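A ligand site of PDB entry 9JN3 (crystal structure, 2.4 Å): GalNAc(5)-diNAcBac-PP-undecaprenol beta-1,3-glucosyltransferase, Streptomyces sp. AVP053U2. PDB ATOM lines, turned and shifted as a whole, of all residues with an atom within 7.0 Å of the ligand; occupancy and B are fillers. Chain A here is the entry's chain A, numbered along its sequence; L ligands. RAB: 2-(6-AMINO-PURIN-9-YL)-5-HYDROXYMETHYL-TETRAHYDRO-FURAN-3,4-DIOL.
The side-chain hydroxyl of Tyr 256 lies within hydrogen-bond range of a nitrogen (N7) of the ligand (2.6 Å).
OG1 of Thr 150 lies within hydrogen-bond range of N6 of the ligand (2.9 Å).
A nitrogen (N1) of the ligand lies within hydrogen-bond range of the side-chain hydroxyl (OH) of Tyr 274.
OH of Tyr 273 lies within hydrogen-bond range of O2' of the ligand (3.5 Å).
The side-chain carboxylate (OE2) of Glu 177 sits at hydrogen-bond distance from a nitrogen (N6) of the ligand.
The side-chain hydroxyl of Thr 150 sits at hydrogen-bond distance from the side-chain hydroxyl of Tyr 274, 2.6 Å away.
The side-chain hydroxyl (OH) of Tyr 274 is in hydrogen-bond range of the backbone carbonyl oxygen (O) of Asn 151, at 2.7 Å.
The backbone NH of Trp 231 lies close to the side-chain carboxylate of Glu 177 (3.4 Å).
The backbone carbonyl oxygen (O) of Val 149 is in hydrogen-bond range of the indole nitrogen (NE1) of Trp 231.
Merely in contact with the ligand: Arg 206 (3.6 Å), Tyr 227 (3.0 Å), Trp 231 (3.6 Å) and Glu 275 (3.7 Å).
Hydrophobic or aromatic side chains that line the ligand: Tyr 227, Trp 231, Tyr 256, Tyr 273 and Tyr 274.
Of the 19 residues printed, 9 come within 4 Å of the ligand.
The nearest printed residue that does not touch the ligand is Leu 224 (4.3 Å).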
ATOM      1  N   VAL A 149      24.971 -17.286 -29.603  1.00  0.00           N
ATOM      2  CA  VAL A 149      24.194 -17.989 -28.589  1.00  0.00           C
ATOM      3  C   VAL A 149      24.725 -17.696 -27.187  1.00  0.00           C
ATOM      4  O   VAL A 149      23.970 -17.368 -26.263  1.00  0.00           O
ATOM      5  CB  VAL A 149      24.205 -19.499 -28.912  1.00  0.00           C
ATOM      6  CG1 VAL A 149      23.360 -20.272 -27.913  1.00  0.00           C
ATOM      7  CG2 VAL A 149      23.717 -19.722 -30.339  1.00  0.00           C
ATOM      8  N   THR A 150      26.036 -17.789 -27.017  1.00  0.00           N
ATOM      9  CA  THR A 150      26.706 -17.560 -25.745  1.00  0.00           C
ATOM     10  C   THR A 150      28.178 -17.584 -26.078  1.00  0.00           C
ATOM     11  O   THR A 150      28.575 -17.922 -27.203  1.00  0.00           O
ATOM     12  CB  THR A 150      26.287 -18.597 -24.681  1.00  0.00           C
ATOM     13  OG1 THR A 150      26.933 -18.346 -23.427  1.00  0.00           O
ATOM     14  CG2 THR A 150      26.626 -20.021 -25.167  1.00  0.00           C
ATOM     15  N   ASN A 151      29.003 -17.219 -25.106  1.00  0.00           N
ATOM     16  CA  ASN A 151      30.425 -17.087 -25.372  1.00  0.00           C
ATOM     17  C   ASN A 151      31.079 -18.451 -25.510  1.00  0.00           C
ATOM     18  O   ASN A 151      30.717 -19.398 -24.825  1.00  0.00           O
ATOM     19  CB  ASN A 151      31.129 -16.279 -24.292  1.00  0.00           C
ATOM     20  CG  ASN A 151      32.459 -15.831 -24.739  1.00  0.00           C
ATOM     21  OD1 ASN A 151      32.871 -16.118 -25.878  1.00  0.00           O
ATOM     22  ND2 ASN A 151      33.179 -15.134 -23.886  1.00  0.00           N
ATOM     23  N   VAL A 176      30.958 -10.079 -14.898  1.00  0.00           N
ATOM     24  CA  VAL A 176      31.103 -11.366 -15.570  1.00  0.00           C
ATOM     25  C   VAL A 176      30.481 -11.261 -16.946  1.00  0.00           C
ATOM     26  O   VAL A 176      29.522 -10.499 -17.162  1.00  0.00           O
ATOM     27  CB  VAL A 176      30.441 -12.542 -14.803  1.00  0.00           C
ATOM     28  CG1 VAL A 176      31.124 -12.754 -13.461  1.00  0.00           C
ATOM     29  CG2 VAL A 176      28.913 -12.320 -14.655  1.00  0.00           C
ATOM     30  N   GLU A 177      30.993 -12.086 -17.859  1.00  0.00           N
ATOM     31  CA  GLU A 177      30.642 -12.024 -19.277  1.00  0.00           C
ATOM     32  C   GLU A 177      30.860 -10.632 -19.864  1.00  0.00           C
ATOM     33  O   GLU A 177      30.161 -10.262 -20.801  1.00  0.00           O
ATOM     34  CB  GLU A 177      29.189 -12.455 -19.522  1.00  0.00           C
ATOM     35  CG  GLU A 177      28.874 -13.948 -19.476  1.00  0.00           C
ATOM     36  CD  GLU A 177      27.385 -14.168 -19.217  1.00  0.00           C
ATOM     37  OE1 GLU A 177      26.983 -14.137 -18.038  1.00  0.00           O
ATOM     38  OE2 GLU A 177      26.599 -14.307 -20.186  1.00  0.00           O
ATOM     39  N   ASP A 179      33.456  -9.967 -21.430  1.00  0.00           N
ATOM     40  CA  ASP A 179      34.151 -10.308 -22.663  1.00  0.00           C
ATOM     41  C   ASP A 179      33.166 -10.680 -23.781  1.00  0.00           C
ATOM     42  O   ASP A 179      33.251 -10.138 -24.902  1.00  0.00           O
ATOM     43  CB  ASP A 179      35.149 -11.425 -22.386  1.00  0.00           C
ATOM     44  CG  ASP A 179      34.526 -12.644 -21.726  1.00  0.00           C
ATOM     45  OD1 ASP A 179      33.476 -12.531 -21.058  1.00  0.00           O
ATOM     46  OD2 ASP A 179      35.114 -13.742 -21.868  1.00  0.00           O
ATOM     47  N   TRP A 180      32.203 -11.565 -23.492  1.00  0.00           N
ATOM     48  CA  TRP A 180      31.116 -11.856 -24.427  1.00  0.00           C
ATOM     49  C   TRP A 180      30.496 -10.569 -24.987  1.00  0.00           C
ATOM     50  O   TRP A 180      30.435 -10.379 -26.218  1.00  0.00           O
ATOM     51  CB  TRP A 180      30.040 -12.730 -23.766  1.00  0.00           C
ATOM     52  CG  TRP A 180      29.140 -13.370 -24.814  1.00  0.00           C
ATOM     53  CD1 TRP A 180      29.527 -13.907 -26.012  1.00  0.00           C
ATOM     54  CD2 TRP A 180      27.697 -13.484 -24.774  1.00  0.00           C
ATOM     55  NE1 TRP A 180      28.433 -14.374 -26.699  1.00  0.00           N
ATOM     56  CE2 TRP A 180      27.303 -14.120 -25.966  1.00  0.00           C
ATOM     57  CE3 TRP A 180      26.718 -13.123 -23.842  1.00  0.00           C
ATOM     58  CZ2 TRP A 180      25.965 -14.386 -26.266  1.00  0.00           C
ATOM     59  CZ3 TRP A 180      25.399 -13.379 -24.148  1.00  0.00           C
ATOM     60  CH2 TRP A 180      25.033 -14.008 -25.357  1.00  0.00           C
ATOM     61  N   ARG A 206      41.908 -22.515 -15.182  1.00  0.00           N
ATOM     62  CA  ARG A 206      40.647 -22.320 -14.475  1.00  0.00           C
ATOM     63  C   ARG A 206      40.610 -23.092 -13.164  1.00  0.00           C
ATOM     64  O   ARG A 206      40.726 -24.322 -13.185  1.00  0.00           O
ATOM     65  CB  ARG A 206      39.467 -22.753 -15.334  1.00  0.00           C
ATOM     66  CG  ARG A 206      39.149 -21.775 -16.414  1.00  0.00           C
ATOM     67  CD  ARG A 206      38.216 -20.657 -15.968  1.00  0.00           C
ATOM     68  NE  ARG A 206      37.156 -20.447 -16.948  1.00  0.00           N
ATOM     69  CZ  ARG A 206      37.089 -19.409 -17.785  1.00  0.00           C
ATOM     70  NH1 ARG A 206      38.026 -18.465 -17.788  1.00  0.00           N
ATOM     71  NH2 ARG A 206      36.081 -19.330 -18.654  1.00  0.00           N
ATOM     72  N   ALA A 223      25.659 -17.295  -7.715  1.00  0.00           N
ATOM     73  CA  ALA A 223      26.731 -17.010  -8.657  1.00  0.00           C
ATOM     74  C   ALA A 223      26.248 -17.170 -10.092  1.00  0.00           C
ATOM     75  O   ALA A 223      26.341 -16.236 -10.908  1.00  0.00           O
ATOM     76  CB  ALA A 223      27.920 -17.929  -8.381  1.00  0.00           C
ATOM     77  N   LEU A 224      25.707 -18.341 -10.402  1.00  0.00           N
ATOM     78  CA  LEU A 224      25.173 -18.614 -11.735  1.00  0.00           C
ATOM     79  C   LEU A 224      24.024 -17.681 -12.088  1.00  0.00           C
ATOM     80  O   LEU A 224      23.762 -17.431 -13.281  1.00  0.00           O
ATOM     81  CB  LEU A 224      24.742 -20.077 -11.790  1.00  0.00           C
ATOM     82  CG  LEU A 224      24.271 -20.606 -13.144  1.00  0.00           C
ATOM     83  CD1 LEU A 224      25.144 -21.727 -13.583  1.00  0.00           C
ATOM     84  CD2 LEU A 224      22.865 -21.145 -13.002  1.00  0.00           C
ATOM     85  N   TYR A 227      25.222 -14.817 -13.822  1.00  0.00           N
ATOM     86  CA  TYR A 227      25.598 -15.164 -15.184  1.00  0.00           C
ATOM     87  C   TYR A 227      24.376 -15.167 -16.104  1.00  0.00           C
ATOM     88  O   TYR A 227      24.363 -14.472 -17.131  1.00  0.00           O
ATOM     89  CB  TYR A 227      26.342 -16.512 -15.161  1.00  0.00           C
ATOM     90  CG  TYR A 227      27.874 -16.375 -14.977  1.00  0.00           C
ATOM     91  CD1 TYR A 227      28.693 -15.956 -16.020  1.00  0.00           C
ATOM     92  CD2 TYR A 227      28.476 -16.645 -13.744  1.00  0.00           C
ATOM     93  CE1 TYR A 227      30.070 -15.816 -15.865  1.00  0.00           C
ATOM     94  CE2 TYR A 227      29.865 -16.506 -13.568  1.00  0.00           C
ATOM     95  CZ  TYR A 227      30.659 -16.082 -14.644  1.00  0.00           C
ATOM     96  OH  TYR A 227      32.025 -15.934 -14.491  1.00  0.00           O
ATOM     97  N   GLU A 228      23.323 -15.907 -15.740  1.00  0.00           N
ATOM     98  CA  GLU A 228      22.079 -15.876 -16.508  1.00  0.00           C
ATOM     99  C   GLU A 228      21.570 -14.460 -16.708  1.00  0.00           C
ATOM    100  O   GLU A 228      21.141 -14.087 -17.808  1.00  0.00           O
ATOM    101  CB  GLU A 228      21.015 -16.737 -15.821  1.00  0.00           C
ATOM    102  CG  GLU A 228      19.562 -16.490 -16.323  1.00  0.00           C
ATOM    103  CD  GLU A 228      18.534 -17.445 -15.708  1.00  0.00           C
ATOM    104  OE1 GLU A 228      18.143 -17.248 -14.530  1.00  0.00           O
ATOM    105  OE2 GLU A 228      18.100 -18.384 -16.413  1.00  0.00           O
ATOM    106  N   TRP A 231      23.795 -12.680 -19.157  1.00  0.00           N
ATOM    107  CA  TRP A 231      23.528 -13.300 -20.447  1.00  0.00           C
ATOM    108  C   TRP A 231      22.224 -12.789 -21.087  1.00  0.00           C
ATOM    109  O   TRP A 231      22.174 -12.577 -22.296  1.00  0.00           O
ATOM    110  CB  TRP A 231      23.516 -14.818 -20.266  1.00  0.00           C
ATOM    111  CG  TRP A 231      23.255 -15.537 -21.556  1.00  0.00           C
ATOM    112  CD1 TRP A 231      24.171 -15.874 -22.493  1.00  0.00           C
ATOM    113  CD2 TRP A 231      21.990 -15.962 -22.056  1.00  0.00           C
ATOM    114  NE1 TRP A 231      23.561 -16.508 -23.552  1.00  0.00           N
ATOM    115  CE2 TRP A 231      22.215 -16.568 -23.293  1.00  0.00           C
ATOM    116  CE3 TRP A 231      20.675 -15.873 -21.570  1.00  0.00           C
ATOM    117  CZ2 TRP A 231      21.182 -17.091 -24.071  1.00  0.00           C
ATOM    118  CZ3 TRP A 231      19.666 -16.404 -22.325  1.00  0.00           C
ATOM    119  CH2 TRP A 231      19.920 -17.000 -23.570  1.00  0.00           C
ATOM    120  N   MET A 252      19.314 -21.871 -23.562  1.00  0.00           N
ATOM    121  CA  MET A 252      20.164 -21.452 -22.452  1.00  0.00           C
ATOM    122  C   MET A 252      19.380 -21.355 -21.152  1.00  0.00           C
ATOM    123  O   MET A 252      19.807 -21.961 -20.155  1.00  0.00           O
ATOM    124  CB  MET A 252      20.896 -20.151 -22.786  1.00  0.00           C
ATOM    125  CG  MET A 252      22.147 -20.349 -23.646  1.00  0.00           C
ATOM    126  SD  MET A 252      23.585 -20.813 -22.666  1.00  0.00           S
ATOM    127  CE  MET A 252      23.571 -22.548 -22.894  1.00  0.00           C
ATOM    128  N   MET A 255      19.054 -24.741 -19.846  1.00  0.00           N
ATOM    129  CA  MET A 255      20.268 -25.208 -19.184  1.00  0.00           C
ATOM    130  C   MET A 255      20.427 -24.597 -17.789  1.00  0.00           C
ATOM    131  O   MET A 255      20.802 -25.289 -16.847  1.00  0.00           O
ATOM    132  CB  MET A 255      21.477 -24.883 -20.070  1.00  0.00           C
ATOM    133  CG  MET A 255      22.788 -25.367 -19.521  1.00  0.00           C
ATOM    134  SD  MET A 255      23.522 -24.019 -18.594  1.00  0.00           S
ATOM    135  CE  MET A 255      25.007 -23.708 -19.535  1.00  0.00           C
ATOM    136  N   TYR A 256      20.131 -23.300 -17.648  1.00  0.00           N
ATOM    137  CA  TYR A 256      20.159 -22.684 -16.331  1.00  0.00           C
ATOM    138  C   TYR A 256      19.181 -23.359 -15.374  1.00  0.00           C
ATOM    139  O   TYR A 256      19.542 -23.754 -14.257  1.00  0.00           O
ATOM    140  CB  TYR A 256      19.851 -21.199 -16.429  1.00  0.00           C
ATOM    141  CG  TYR A 256      20.992 -20.405 -17.015  1.00  0.00           C
ATOM    142  CD1 TYR A 256      22.305 -20.715 -16.691  1.00  0.00           C
ATOM    143  CD2 TYR A 256      20.765 -19.372 -17.921  1.00  0.00           C
ATOM    144  CE1 TYR A 256      23.347 -20.009 -17.226  1.00  0.00           C
ATOM    145  CE2 TYR A 256      21.825 -18.656 -18.463  1.00  0.00           C
ATOM    146  CZ  TYR A 256      23.113 -18.973 -18.099  1.00  0.00           C
ATOM    147  OH  TYR A 256      24.177 -18.270 -18.624  1.00  0.00           O
ATOM    148  N   TYR A 273      30.584 -28.250 -17.159  1.00  0.00           N
ATOM    149  CA  TYR A 273      29.265 -28.442 -17.739  1.00  0.00           C
ATOM    150  C   TYR A 273      28.947 -27.371 -18.785  1.00  0.00           C
ATOM    151  O   TYR A 273      28.248 -27.663 -19.771  1.00  0.00           O
ATOM    152  CB  TYR A 273      28.208 -28.458 -16.646  1.00  0.00           C
ATOM    153  CG  TYR A 273      27.986 -27.154 -15.940  1.00  0.00           C
ATOM    154  CD1 TYR A 273      27.081 -26.220 -16.429  1.00  0.00           C
ATOM    155  CD2 TYR A 273      28.661 -26.863 -14.752  1.00  0.00           C
ATOM    156  CE1 TYR A 273      26.868 -25.025 -15.774  1.00  0.00           C
ATOM    157  CE2 TYR A 273      28.459 -25.676 -14.094  1.00  0.00           C
ATOM    158  CZ  TYR A 273      27.562 -24.755 -14.612  1.00  0.00           C
ATOM    159  OH  TYR A 273      27.350 -23.569 -13.952  1.00  0.00           O
ATOM    160  N   TYR A 274      29.441 -26.140 -18.574  1.00  0.00           N
ATOM    161  CA  TYR A 274      29.300 -25.116 -19.596  1.00  0.00           C
ATOM    162  C   TYR A 274      29.991 -25.531 -20.894  1.00  0.00           C
ATOM    163  O   TYR A 274      29.408 -25.449 -21.987  1.00  0.00           O
ATOM    164  CB  TYR A 274      29.871 -23.791 -19.072  1.00  0.00           C
ATOM    165  CG  TYR A 274      29.720 -22.643 -20.038  1.00  0.00           C
ATOM    166  CD1 TYR A 274      30.691 -22.377 -20.994  1.00  0.00           C
ATOM    167  CD2 TYR A 274      28.589 -21.855 -20.005  1.00  0.00           C
ATOM    168  CE1 TYR A 274      30.544 -21.317 -21.887  1.00  0.00           C
ATOM    169  CE2 TYR A 274      28.418 -20.820 -20.873  1.00  0.00           C
ATOM    170  CZ  TYR A 274      29.389 -20.549 -21.820  1.00  0.00           C
ATOM    171  OH  TYR A 274      29.158 -19.492 -22.670  1.00  0.00           O
ATOM    172  N   GLU A 275      31.240 -26.000 -20.810  1.00  0.00           N
ATOM    173  CA  GLU A 275      31.974 -26.385 -22.004  1.00  0.00           C
ATOM    174  C   GLU A 275      31.382 -27.626 -22.653  1.00  0.00           C
ATOM    175  O   GLU A 275      31.420 -27.763 -23.877  1.00  0.00           O
ATOM    176  CB  GLU A 275      33.453 -26.597 -21.676  1.00  0.00           C
ATOM    177  CG  GLU A 275      34.225 -25.304 -21.324  1.00  0.00           C
ATOM    178  CD  GLU A 275      33.968 -24.760 -19.900  1.00  0.00           C
ATOM    179  OE1 GLU A 275      33.712 -25.555 -18.953  1.00  0.00           O
ATOM    180  OE2 GLU A 275      34.034 -23.523 -19.713  1.00  0.00           O
HETATM  181  O5' RAB L   1      33.136 -20.870 -17.279  1.00  0.00           O
HETATM  182  C5' RAB L   1      31.842 -20.360 -16.990  1.00  0.00           C
HETATM  183  C4' RAB L   1      31.522 -19.945 -15.566  1.00  0.00           C
HETATM  184  O4' RAB L   1      30.471 -18.948 -15.604  1.00  0.00           O
HETATM  185  C1' RAB L   1      29.217 -19.624 -15.514  1.00  0.00           C
HETATM  186  N9  RAB L   1      28.379 -19.297 -16.682  1.00  0.00           N
HETATM  187  C4  RAB L   1      28.735 -18.667 -17.850  1.00  0.00           C
HETATM  188  N3  RAB L   1      29.953 -18.240 -18.242  1.00  0.00           N
HETATM  189  C2  RAB L   1      29.904 -17.674 -19.449  1.00  0.00           C
HETATM  190  N1  RAB L   1      28.849 -17.507 -20.255  1.00  0.00           N
HETATM  191  C6  RAB L   1      27.635 -17.935 -19.841  1.00  0.00           C
HETATM  192  N6  RAB L   1      26.581 -17.750 -20.633  1.00  0.00           N
HETATM  193  C5  RAB L   1      27.561 -18.549 -18.588  1.00  0.00           C
HETATM  194  N7  RAB L   1      26.492 -19.093 -17.881  1.00  0.00           N
HETATM  195  C8  RAB L   1      27.027 -19.510 -16.761  1.00  0.00           C
HETATM  196  C2' RAB L   1      29.477 -21.091 -15.164  1.00  0.00           C
HETATM  197  O2' RAB L   1      29.284 -21.916 -16.290  1.00  0.00           O
HETATM  198  C3' RAB L   1      30.924 -21.012 -14.646  1.00  0.00           C
HETATM  199  O3' RAB L   1      30.864 -20.463 -13.333  1.00  0.00           O
